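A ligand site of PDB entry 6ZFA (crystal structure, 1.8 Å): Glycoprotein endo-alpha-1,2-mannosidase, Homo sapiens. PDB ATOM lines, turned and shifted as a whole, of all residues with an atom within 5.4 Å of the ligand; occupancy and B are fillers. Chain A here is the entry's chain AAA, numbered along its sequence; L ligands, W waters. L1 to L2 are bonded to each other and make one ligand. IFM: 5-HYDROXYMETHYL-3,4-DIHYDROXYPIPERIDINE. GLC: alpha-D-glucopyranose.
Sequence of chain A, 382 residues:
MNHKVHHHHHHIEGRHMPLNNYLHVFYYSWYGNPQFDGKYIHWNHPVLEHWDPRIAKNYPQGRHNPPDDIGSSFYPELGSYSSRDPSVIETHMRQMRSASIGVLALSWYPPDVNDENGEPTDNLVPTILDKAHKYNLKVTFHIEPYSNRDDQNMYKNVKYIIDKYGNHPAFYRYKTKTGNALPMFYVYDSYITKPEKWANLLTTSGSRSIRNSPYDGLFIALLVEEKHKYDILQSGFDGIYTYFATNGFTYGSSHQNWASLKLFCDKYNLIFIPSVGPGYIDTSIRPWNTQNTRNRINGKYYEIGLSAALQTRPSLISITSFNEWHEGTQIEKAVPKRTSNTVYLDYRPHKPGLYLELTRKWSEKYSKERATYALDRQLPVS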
ATOM      1  N   TYR A  28     -38.018 -13.865  15.901  1.00  0.00           N
ATOM      2  CA  TYR A  28     -36.760 -14.152  16.579  1.00  0.00           C
ATOM      3  C   TYR A  28     -37.087 -14.707  17.971  1.00  0.00           C
ATOM      4  O   TYR A  28     -37.871 -14.100  18.698  1.00  0.00           O
ATOM      5  CB  TYR A  28     -35.886 -12.876  16.630  1.00  0.00           C
ATOM      6  CG  TYR A  28     -35.504 -12.509  15.221  1.00  0.00           C
ATOM      7  CD1 TYR A  28     -36.376 -11.757  14.415  1.00  0.00           C
ATOM      8  CD2 TYR A  28     -34.332 -13.020  14.642  1.00  0.00           C
ATOM      9  CE1 TYR A  28     -36.074 -11.499  13.098  1.00  0.00           C
ATOM     10  CE2 TYR A  28     -33.999 -12.744  13.314  1.00  0.00           C
ATOM     11  CZ  TYR A  28     -34.889 -12.009  12.547  1.00  0.00           C
ATOM     12  OH  TYR A  28     -34.578 -11.747  11.233  1.00  0.00           O
ATOM     13  N   TRP A  30     -34.517 -15.489  20.317  1.00  0.00           N
ATOM     14  CA  TRP A  30     -33.222 -15.491  20.961  1.00  0.00           C
ATOM     15  C   TRP A  30     -33.064 -14.589  22.217  1.00  0.00           C
ATOM     16  O   TRP A  30     -31.945 -14.422  22.702  1.00  0.00           O
ATOM     17  CB  TRP A  30     -32.146 -15.167  19.938  1.00  0.00           C
ATOM     18  CG  TRP A  30     -32.301 -13.826  19.241  1.00  0.00           C
ATOM     19  CD1 TRP A  30     -33.012 -12.716  19.674  1.00  0.00           C
ATOM     20  CD2 TRP A  30     -31.707 -13.452  17.997  1.00  0.00           C
ATOM     21  NE1 TRP A  30     -32.891 -11.702  18.752  1.00  0.00           N
ATOM     22  CE2 TRP A  30     -32.073 -12.110  17.734  1.00  0.00           C
ATOM     23  CE3 TRP A  30     -30.850 -14.113  17.079  1.00  0.00           C
ATOM     24  CZ2 TRP A  30     -31.663 -11.419  16.576  1.00  0.00           C
ATOM     25  CZ3 TRP A  30     -30.437 -13.418  15.938  1.00  0.00           C
ATOM     26  CH2 TRP A  30     -30.861 -12.088  15.691  1.00  0.00           C
ATOM     27  N   HIS A  42     -29.216 -11.391  24.581  1.00  0.00           N
ATOM     28  CA  HIS A  42     -29.543 -10.434  23.504  1.00  0.00           C
ATOM     29  C   HIS A  42     -29.919  -9.018  23.949  1.00  0.00           C
ATOM     30  O   HIS A  42     -29.429  -8.056  23.364  1.00  0.00           O
ATOM     31  CB  HIS A  42     -30.562 -11.033  22.493  1.00  0.00           C
ATOM     32  CG  HIS A  42     -29.921 -11.818  21.403  1.00  0.00           C
ATOM     33  ND1 HIS A  42     -29.653 -11.279  20.155  1.00  0.00           N
ATOM     34  CD2 HIS A  42     -29.473 -13.101  21.348  1.00  0.00           C
ATOM     35  CE1 HIS A  42     -29.077 -12.199  19.397  1.00  0.00           C
ATOM     36  NE2 HIS A  42     -28.946 -13.304  20.097  1.00  0.00           N
ATOM     37  N   HIS A  45     -26.852  -6.975  24.526  1.00  0.00           N
ATOM     38  CA  HIS A  45     -26.064  -7.149  23.314  1.00  0.00           C
ATOM     39  C   HIS A  45     -24.803  -6.295  23.386  1.00  0.00           C
ATOM     40  O   HIS A  45     -24.828  -5.155  23.898  1.00  0.00           O
ATOM     41  CB  HIS A  45     -26.862  -6.712  22.069  1.00  0.00           C
ATOM     42  CG  HIS A  45     -26.416  -7.364  20.791  1.00  0.00           C
ATOM     43  ND1 HIS A  45     -25.291  -6.969  20.104  1.00  0.00           N
ATOM     44  CD2 HIS A  45     -27.017  -8.301  20.016  1.00  0.00           C
ATOM     45  CE1 HIS A  45     -25.180  -7.685  18.993  1.00  0.00           C
ATOM     46  NE2 HIS A  45     -26.223  -8.496  18.905  1.00  0.00           N
ATOM     47  N   LEU A  48     -21.231  -3.638  18.507  1.00  0.00           N
ATOM     48  CA  LEU A  48     -20.402  -4.279  17.488  1.00  0.00           C
ATOM     49  C   LEU A  48     -19.357  -3.302  17.009  1.00  0.00           C
ATOM     50  O   LEU A  48     -19.669  -2.173  16.670  1.00  0.00           O
ATOM     51  CB  LEU A  48     -21.267  -4.794  16.338  1.00  0.00           C
ATOM     52  CG  LEU A  48     -22.276  -5.861  16.794  1.00  0.00           C
ATOM     53  CD1 LEU A  48     -23.155  -6.405  15.684  1.00  0.00           C
ATOM     54  CD2 LEU A  48     -21.676  -7.039  17.591  1.00  0.00           C
ATOM     55  N   SER A 107     -36.428 -17.529  12.871  1.00  0.00           N
ATOM     56  CA  SER A 107     -34.955 -17.553  12.826  1.00  0.00           C
ATOM     57  C   SER A 107     -34.434 -18.834  13.495  1.00  0.00           C
ATOM     58  O   SER A 107     -34.854 -19.176  14.609  1.00  0.00           O
ATOM     59  CB  SER A 107     -34.351 -16.268  13.463  1.00  0.00           C
ATOM     60  OG  SER A 107     -32.966 -16.350  13.657  1.00  0.00           O
ATOM     61  N   TYR A 109     -31.104 -21.769  14.072  1.00  0.00           N
ATOM     62  CA  TYR A 109     -29.799 -22.395  14.012  1.00  0.00           C
ATOM     63  C   TYR A 109     -29.968 -23.882  14.360  1.00  0.00           C
ATOM     64  O   TYR A 109     -30.884 -24.258  15.051  1.00  0.00           O
ATOM     65  CB  TYR A 109     -28.855 -21.745  15.041  1.00  0.00           C
ATOM     66  CG  TYR A 109     -28.259 -20.439  14.539  1.00  0.00           C
ATOM     67  CD1 TYR A 109     -28.962 -19.226  14.679  1.00  0.00           C
ATOM     68  CD2 TYR A 109     -27.017 -20.400  13.929  1.00  0.00           C
ATOM     69  CE1 TYR A 109     -28.417 -18.024  14.220  1.00  0.00           C
ATOM     70  CE2 TYR A 109     -26.468 -19.194  13.487  1.00  0.00           C
ATOM     71  CZ  TYR A 109     -27.192 -18.019  13.634  1.00  0.00           C
ATOM     72  OH  TYR A 109     -26.654 -16.831  13.149  1.00  0.00           O
ATOM     73  N   ASP A 115     -26.497 -18.116  17.205  1.00  0.00           N
ATOM     74  CA  ASP A 115     -25.939 -16.868  16.720  1.00  0.00           C
ATOM     75  C   ASP A 115     -24.786 -16.488  17.663  1.00  0.00           C
ATOM     76  O   ASP A 115     -24.695 -16.943  18.813  1.00  0.00           O
ATOM     77  CB  ASP A 115     -27.015 -15.785  16.591  1.00  0.00           C
ATOM     78  CG  ASP A 115     -27.274 -15.028  17.894  1.00  0.00           C
ATOM     79  OD1 ASP A 115     -28.065 -15.530  18.739  1.00  0.00           O
ATOM     80  OD2 ASP A 115     -26.660 -13.928  18.044  1.00  0.00           O
ATOM     81  N   GLU A 116     -23.889 -15.679  17.159  1.00  0.00           N
ATOM     82  CA  GLU A 116     -22.661 -15.351  17.873  1.00  0.00           C
ATOM     83  C   GLU A 116     -22.901 -14.481  19.115  1.00  0.00           C
ATOM     84  O   GLU A 116     -22.018 -14.323  19.934  1.00  0.00           O
ATOM     85  CB  GLU A 116     -21.662 -14.695  16.910  1.00  0.00           C
ATOM     86  CG  GLU A 116     -22.162 -13.433  16.211  1.00  0.00           C
ATOM     87  CD  GLU A 116     -22.931 -13.648  14.883  1.00  0.00           C
ATOM     88  OE1 GLU A 116     -22.805 -12.735  14.032  1.00  0.00           O
ATOM     89  OE2 GLU A 116     -23.672 -14.688  14.692  1.00  0.00           O
ATOM     90  N   ASN A 117     -24.102 -13.924  19.259  1.00  0.00           N
ATOM     91  CA  ASN A 117     -24.456 -13.124  20.427  1.00  0.00           C
ATOM     92  C   ASN A 117     -25.519 -13.759  21.291  1.00  0.00           C
ATOM     93  O   ASN A 117     -26.069 -13.099  22.129  1.00  0.00           O
ATOM     94  CB  ASN A 117     -24.898 -11.717  19.985  1.00  0.00           C
ATOM     95  CG  ASN A 117     -23.806 -10.957  19.267  1.00  0.00           C
ATOM     96  OD1 ASN A 117     -23.832 -10.771  18.046  1.00  0.00           O
ATOM     97  ND2 ASN A 117     -22.790 -10.558  20.029  1.00  0.00           N
ATOM     98  N   HIS A 142     -36.385 -19.873   8.939  1.00  0.00           N
ATOM     99  CA  HIS A 142     -35.483 -18.867   8.405  1.00  0.00           C
ATOM    100  C   HIS A 142     -34.085 -19.311   8.804  1.00  0.00           C
ATOM    101  O   HIS A 142     -33.614 -19.045   9.912  1.00  0.00           O
ATOM    102  CB  HIS A 142     -35.844 -17.475   8.962  1.00  0.00           C
ATOM    103  CG  HIS A 142     -35.100 -16.325   8.313  1.00  0.00           C
ATOM    104  ND1 HIS A 142     -35.083 -15.053   8.833  1.00  0.00           N
ATOM    105  CD2 HIS A 142     -34.379 -16.264   7.157  1.00  0.00           C
ATOM    106  CE1 HIS A 142     -34.387 -14.266   8.033  1.00  0.00           C
ATOM    107  NE2 HIS A 142     -33.945 -14.972   7.011  1.00  0.00           N
ATOM    108  N   GLU A 144     -30.381 -19.532   9.330  1.00  0.00           N
ATOM    109  CA  GLU A 144     -29.347 -18.539   9.534  1.00  0.00           C
ATOM    110  C   GLU A 144     -28.003 -19.064   9.036  1.00  0.00           C
ATOM    111  O   GLU A 144     -27.882 -20.266   8.772  1.00  0.00           O
ATOM    112  CB  GLU A 144     -29.320 -18.140  11.017  1.00  0.00           C
ATOM    113  CG  GLU A 144     -30.608 -17.493  11.529  1.00  0.00           C
ATOM    114  CD  GLU A 144     -30.746 -16.006  11.140  1.00  0.00           C
ATOM    115  OE1 GLU A 144     -29.851 -15.504  10.479  1.00  0.00           O
ATOM    116  OE2 GLU A 144     -31.747 -15.339  11.511  1.00  0.00           O
ATOM    117  N   PRO A 145     -27.006 -18.175   8.849  1.00  0.00           N
ATOM    118  CA  PRO A 145     -25.709 -18.596   8.293  1.00  0.00           C
ATOM    119  C   PRO A 145     -24.772 -19.081   9.380  1.00  0.00           C
ATOM    120  O   PRO A 145     -23.882 -18.375   9.812  1.00  0.00           O
ATOM    121  CB  PRO A 145     -25.191 -17.352   7.581  1.00  0.00           C
ATOM    122  CG  PRO A 145     -25.924 -16.209   8.187  1.00  0.00           C
ATOM    123  CD  PRO A 145     -27.046 -16.717   9.027  1.00  0.00           C
ATOM    124  N   TYR A 188     -31.045 -17.267   4.794  1.00  0.00           N
ATOM    125  CA  TYR A 188     -30.373 -15.981   4.972  1.00  0.00           C
ATOM    126  C   TYR A 188     -28.897 -16.030   4.551  1.00  0.00           C
ATOM    127  O   TYR A 188     -28.148 -16.942   4.918  1.00  0.00           O
ATOM    128  CB  TYR A 188     -30.496 -15.457   6.404  1.00  0.00           C
ATOM    129  CG  TYR A 188     -29.968 -14.022   6.512  1.00  0.00           C
ATOM    130  CD1 TYR A 188     -30.705 -12.943   6.012  1.00  0.00           C
ATOM    131  CD2 TYR A 188     -28.730 -13.761   7.064  1.00  0.00           C
ATOM    132  CE1 TYR A 188     -30.199 -11.647   6.067  1.00  0.00           C
ATOM    133  CE2 TYR A 188     -28.229 -12.478   7.147  1.00  0.00           C
ATOM    134  CZ  TYR A 188     -28.956 -11.419   6.644  1.00  0.00           C
ATOM    135  OH  TYR A 188     -28.404 -10.150   6.701  1.00  0.00           O
ATOM    136  N   TYR A 243     -35.254  -9.338   2.364  1.00  0.00           N
ATOM    137  CA  TYR A 243     -35.077  -9.124   3.822  1.00  0.00           C
ATOM    138  C   TYR A 243     -35.023  -7.664   4.331  1.00  0.00           C
ATOM    139  O   TYR A 243     -35.859  -7.278   5.146  1.00  0.00           O
ATOM    140  CB  TYR A 243     -33.948  -9.972   4.454  1.00  0.00           C
ATOM    141  CG  TYR A 243     -34.014  -9.861   5.941  1.00  0.00           C
ATOM    142  CD1 TYR A 243     -34.899 -10.655   6.670  1.00  0.00           C
ATOM    143  CD2 TYR A 243     -33.254  -8.899   6.632  1.00  0.00           C
ATOM    144  CE1 TYR A 243     -35.011 -10.533   8.049  1.00  0.00           C
ATOM    145  CE2 TYR A 243     -33.381  -8.737   8.005  1.00  0.00           C
ATOM    146  CZ  TYR A 243     -34.255  -9.531   8.707  1.00  0.00           C
ATOM    147  OH  TYR A 243     -34.334  -9.338  10.068  1.00  0.00           O
ATOM    148  N   ILE A 285     -26.377  -0.933  18.626  1.00  0.00           N
ATOM    149  CA  ILE A 285     -25.377  -2.010  18.431  1.00  0.00           C
ATOM    150  C   ILE A 285     -24.438  -1.806  17.266  1.00  0.00           C
ATOM    151  O   ILE A 285     -23.362  -2.404  17.257  1.00  0.00           O
ATOM    152  CB  ILE A 285     -25.996  -3.402  18.388  1.00  0.00           C
ATOM    153  CG1 ILE A 285     -26.915  -3.587  17.177  1.00  0.00           C
ATOM    154  CG2 ILE A 285     -26.741  -3.677  19.703  1.00  0.00           C
ATOM    155  CD1 ILE A 285     -26.929  -4.999  16.629  1.00  0.00           C
ATOM    156  N   ARG A 286     -24.822  -0.993  16.290  1.00  0.00           N
ATOM    157  CA  ARG A 286     -23.954  -0.640  15.173  1.00  0.00           C
ATOM    158  C   ARG A 286     -23.931   0.893  15.034  1.00  0.00           C
ATOM    159  O   ARG A 286     -24.483   1.455  14.094  1.00  0.00           O
ATOM    160  CB  ARG A 286     -24.387  -1.349  13.870  1.00  0.00           C
ATOM    161  CG  ARG A 286     -24.418  -2.877  13.960  1.00  0.00           C
ATOM    162  CD  ARG A 286     -24.573  -3.529  12.590  1.00  0.00           C
ATOM    163  NE  ARG A 286     -24.957  -4.925  12.726  1.00  0.00           N
ATOM    164  CZ  ARG A 286     -26.201  -5.408  12.786  1.00  0.00           C
ATOM    165  NH1 ARG A 286     -27.287  -4.622  12.692  1.00  0.00           N
ATOM    166  NH2 ARG A 286     -26.361  -6.723  12.939  1.00  0.00           N
ATOM    167  N   GLU A 324     -37.118  -8.082  15.552  1.00  0.00           N
ATOM    168  CA  GLU A 324     -35.664  -7.800  15.505  1.00  0.00           C
ATOM    169  C   GLU A 324     -35.488  -6.387  16.145  1.00  0.00           C
ATOM    170  O   GLU A 324     -35.487  -5.349  15.479  1.00  0.00           O
ATOM    171  CB  GLU A 324     -35.098  -7.915  14.079  1.00  0.00           C
ATOM    172  CG  GLU A 324     -33.722  -8.606  13.965  1.00  0.00           C
ATOM    173  CD  GLU A 324     -32.575  -7.902  14.699  1.00  0.00           C
ATOM    174  OE1 GLU A 324     -31.415  -8.265  14.469  1.00  0.00           O
ATOM    175  OE2 GLU A 324     -32.804  -6.997  15.536  1.00  0.00           O
ATOM    176  N   HIS A 326     -32.953  -5.165  17.834  1.00  0.00           N
ATOM    177  CA  HIS A 326     -31.611  -4.545  17.629  1.00  0.00           C
ATOM    178  C   HIS A 326     -31.609  -3.626  16.428  1.00  0.00           C
ATOM    179  O   HIS A 326     -30.973  -2.592  16.443  1.00  0.00           O
ATOM    180  CB  HIS A 326     -30.519  -5.581  17.416  1.00  0.00           C
ATOM    181  CG  HIS A 326     -30.542  -6.672  18.444  1.00  0.00           C
ATOM    182  ND1 HIS A 326     -30.497  -6.403  19.791  1.00  0.00           N
ATOM    183  CD2 HIS A 326     -30.644  -8.015  18.324  1.00  0.00           C
ATOM    184  CE1 HIS A 326     -30.531  -7.536  20.467  1.00  0.00           C
ATOM    185  NE2 HIS A 326     -30.623  -8.530  19.607  1.00  0.00           N
ATOM    186  N   GLU A 327     -32.331  -4.038  15.392  1.00  0.00           N
ATOM    187  CA  GLU A 327     -32.344  -3.313  14.118  1.00  0.00           C
ATOM    188  C   GLU A 327     -33.501  -2.369  13.936  1.00  0.00           C
ATOM    189  O   GLU A 327     -33.598  -1.671  12.888  1.00  0.00           O
ATOM    190  CB  GLU A 327     -32.246  -4.327  12.990  1.00  0.00           C
ATOM    191  CG  GLU A 327     -30.932  -5.083  13.057  1.00  0.00           C
ATOM    192  CD  GLU A 327     -30.657  -6.033  11.905  1.00  0.00           C
ATOM    193  OE1 GLU A 327     -31.584  -6.545  11.283  1.00  0.00           O
ATOM    194  OE2 GLU A 327     -29.461  -6.279  11.658  1.00  0.00           O
HETATM  195  O4  IFM L   1     -28.779 -13.085  10.756  1.00  0.00           O
HETATM  196  C4  IFM L   1     -29.653 -12.075  11.248  1.00  0.00           C
HETATM  197  C3  IFM L   1     -28.766 -10.942  11.834  1.00  0.00           C
HETATM  198  O3  IFM L   1     -28.020 -11.475  12.932  1.00  0.00           O
HETATM  199  C2  IFM L   1     -29.611  -9.738  12.269  1.00  0.00           C
HETATM  200  N   IFM L   1     -30.498  -9.372  11.187  1.00  0.00           N
HETATM  201  C1  IFM L   1     -31.382 -10.371  10.623  1.00  0.00           C
HETATM  202  C5  IFM L   1     -30.567 -11.557  10.125  1.00  0.00           C
HETATM  203  C6  IFM L   1     -31.535 -12.571   9.522  1.00  0.00           C
HETATM  204  O6  IFM L   1     -32.416 -13.158  10.492  1.00  0.00           O
HETATM  205  C1  GLC L   2     -26.831 -10.729  13.227  1.00  0.00           C
HETATM  206  C2  GLC L   2     -25.936 -11.568  14.104  1.00  0.00           C
HETATM  207  C3  GLC L   2     -26.551 -11.699  15.489  1.00  0.00           C
HETATM  208  C4  GLC L   2     -26.806 -10.301  16.063  1.00  0.00           C
HETATM  209  C5  GLC L   2     -27.723  -9.525  15.134  1.00  0.00           C
HETATM  210  C6  GLC L   2     -27.940  -8.081  15.616  1.00  0.00           C
HETATM  211  O2  GLC L   2     -25.778 -12.858  13.477  1.00  0.00           O
HETATM  212  O3  GLC L   2     -25.602 -12.452  16.242  1.00  0.00           O
HETATM  213  O4  GLC L   2     -27.359 -10.452  17.367  1.00  0.00           O
HETATM  214  O5  GLC L   2     -27.078  -9.450  13.858  1.00  0.00           O
HETATM  215  O6  GLC L   2     -28.780  -7.385  14.671  1.00  0.00           O
HETATM  216  O   HOH W   1     -29.379  -8.510   8.716  1.00  0.00           O
HETATM  217  O   HOH W   2     -26.101 -12.982  10.677  1.00  0.00           O
HETATM  218  O   HOH W   3     -23.744 -11.662  11.897  1.00  0.00           O
HETATM  219  O   HOH W   4     -28.078 -14.587  13.288  1.00  0.00           O
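The side-chain carboxylate (OD2) of Asp 115 is in hydrogen-bond range of an oxygen (O3) of GLC L2 (2.6 Å).
A ring nitrogen (NE2) of His 45 lies within hydrogen-bond range of an oxygen (O4) of GLC L2.
The guanidinium group of Arg 286 is in hydrogen-bond range of an oxygen (O5) of GLC L2 (3.0 Å).
The side-chain carboxylate (OE1) of Glu 116 is in hydrogen-bond range of an oxygen (O2) of GLC L2 (3.0 Å).
OD1 of Asn 117 sits at hydrogen-bond distance from O3 of GLC L2 (3.0 Å).
A nitrogen (N) of IFM L1 lies within salt-bridge range of the side-chain carboxylate (OE1) of Glu 324, at 3.6 Å.
OE1 of Glu 327 is in salt-bridge range of N of IFM L1.
An oxygen (O6) of IFM L1 is in hydrogen-bond range of the side-chain hydroxyl (OH) of Tyr 28 (2.7 Å).
OE2 of Glu 144 lies within hydrogen-bond range of O6 of IFM L1, at 2.5 Å.
His 42 touches the ligand.
CE1 of His 142 touches O6 of IFM L1 (3.3 Å).
CD1 of Tyr 188 touches C6 of IFM L1 (3.6 Å).
Tyr 243 touches the ligand.
CD1 of Ile 285 touches C6 of GLC L2, 3.4 Å away.
CB of His 326 touches O6 of GLC L2, at 3.7 Å.
15 residues have an atom within 4 Å of the ligand: Tyr 28, His 42, His 45, Asp 115, Glu 116, Asn 117, His 142, Glu 144, Tyr 188, Tyr 243, Ile 285, Arg 286, Glu 324, His 326 and Glu 327.
The side-chain carboxylate of Asp 115 lies within hydrogen-bond range of a ring nitrogen (NE2) of His 42.
The side-chain carboxylate (OE2) of Glu 324 sits at hydrogen-bond distance from the backbone NH (N) of Glu 327 (3.0 Å).
The backbone NH of His 326 is in hydrogen-bond range of the side-chain carboxylate of Glu 324, at 2.9 Å.
NE2 of His 45 is in hydrogen-bond range of OD1 of Asn 117, at 3.4 Å.
N of Leu 48 is in hydrogen-bond range of O of Ile 285 (2.8 Å).
The side-chain carboxylate (OD2) of Asp 115 sits at hydrogen-bond distance from the backbone NH (N) of Asn 117, at 2.8 Å.
The side-chain hydroxyl (OH) of Tyr 243 lies within hydrogen-bond range of the side-chain hydroxyl (OH) of Tyr 28, 2.7 Å away.
The side-chain hydroxyl (OG) of Ser 107 is in hydrogen-bond range of the side-chain carboxylate (OE2) of Glu 144 (2.7 Å).
Water W3 bridges OE1 of Glu 116 (2.6 Å) and O2 of GLC L2 (2.8 Å).
Water W1 lies within hydrogen-bond range of the side-chain hydroxyl (OH) of Tyr 188 and a nitrogen (N) of IFM L1.
Water W4 lies within hydrogen-bond range of OH of Tyr 109 (2.7 Å), O2 of GLC L2 (2.9 Å) and OE1 of Glu 144 (3.4 Å).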
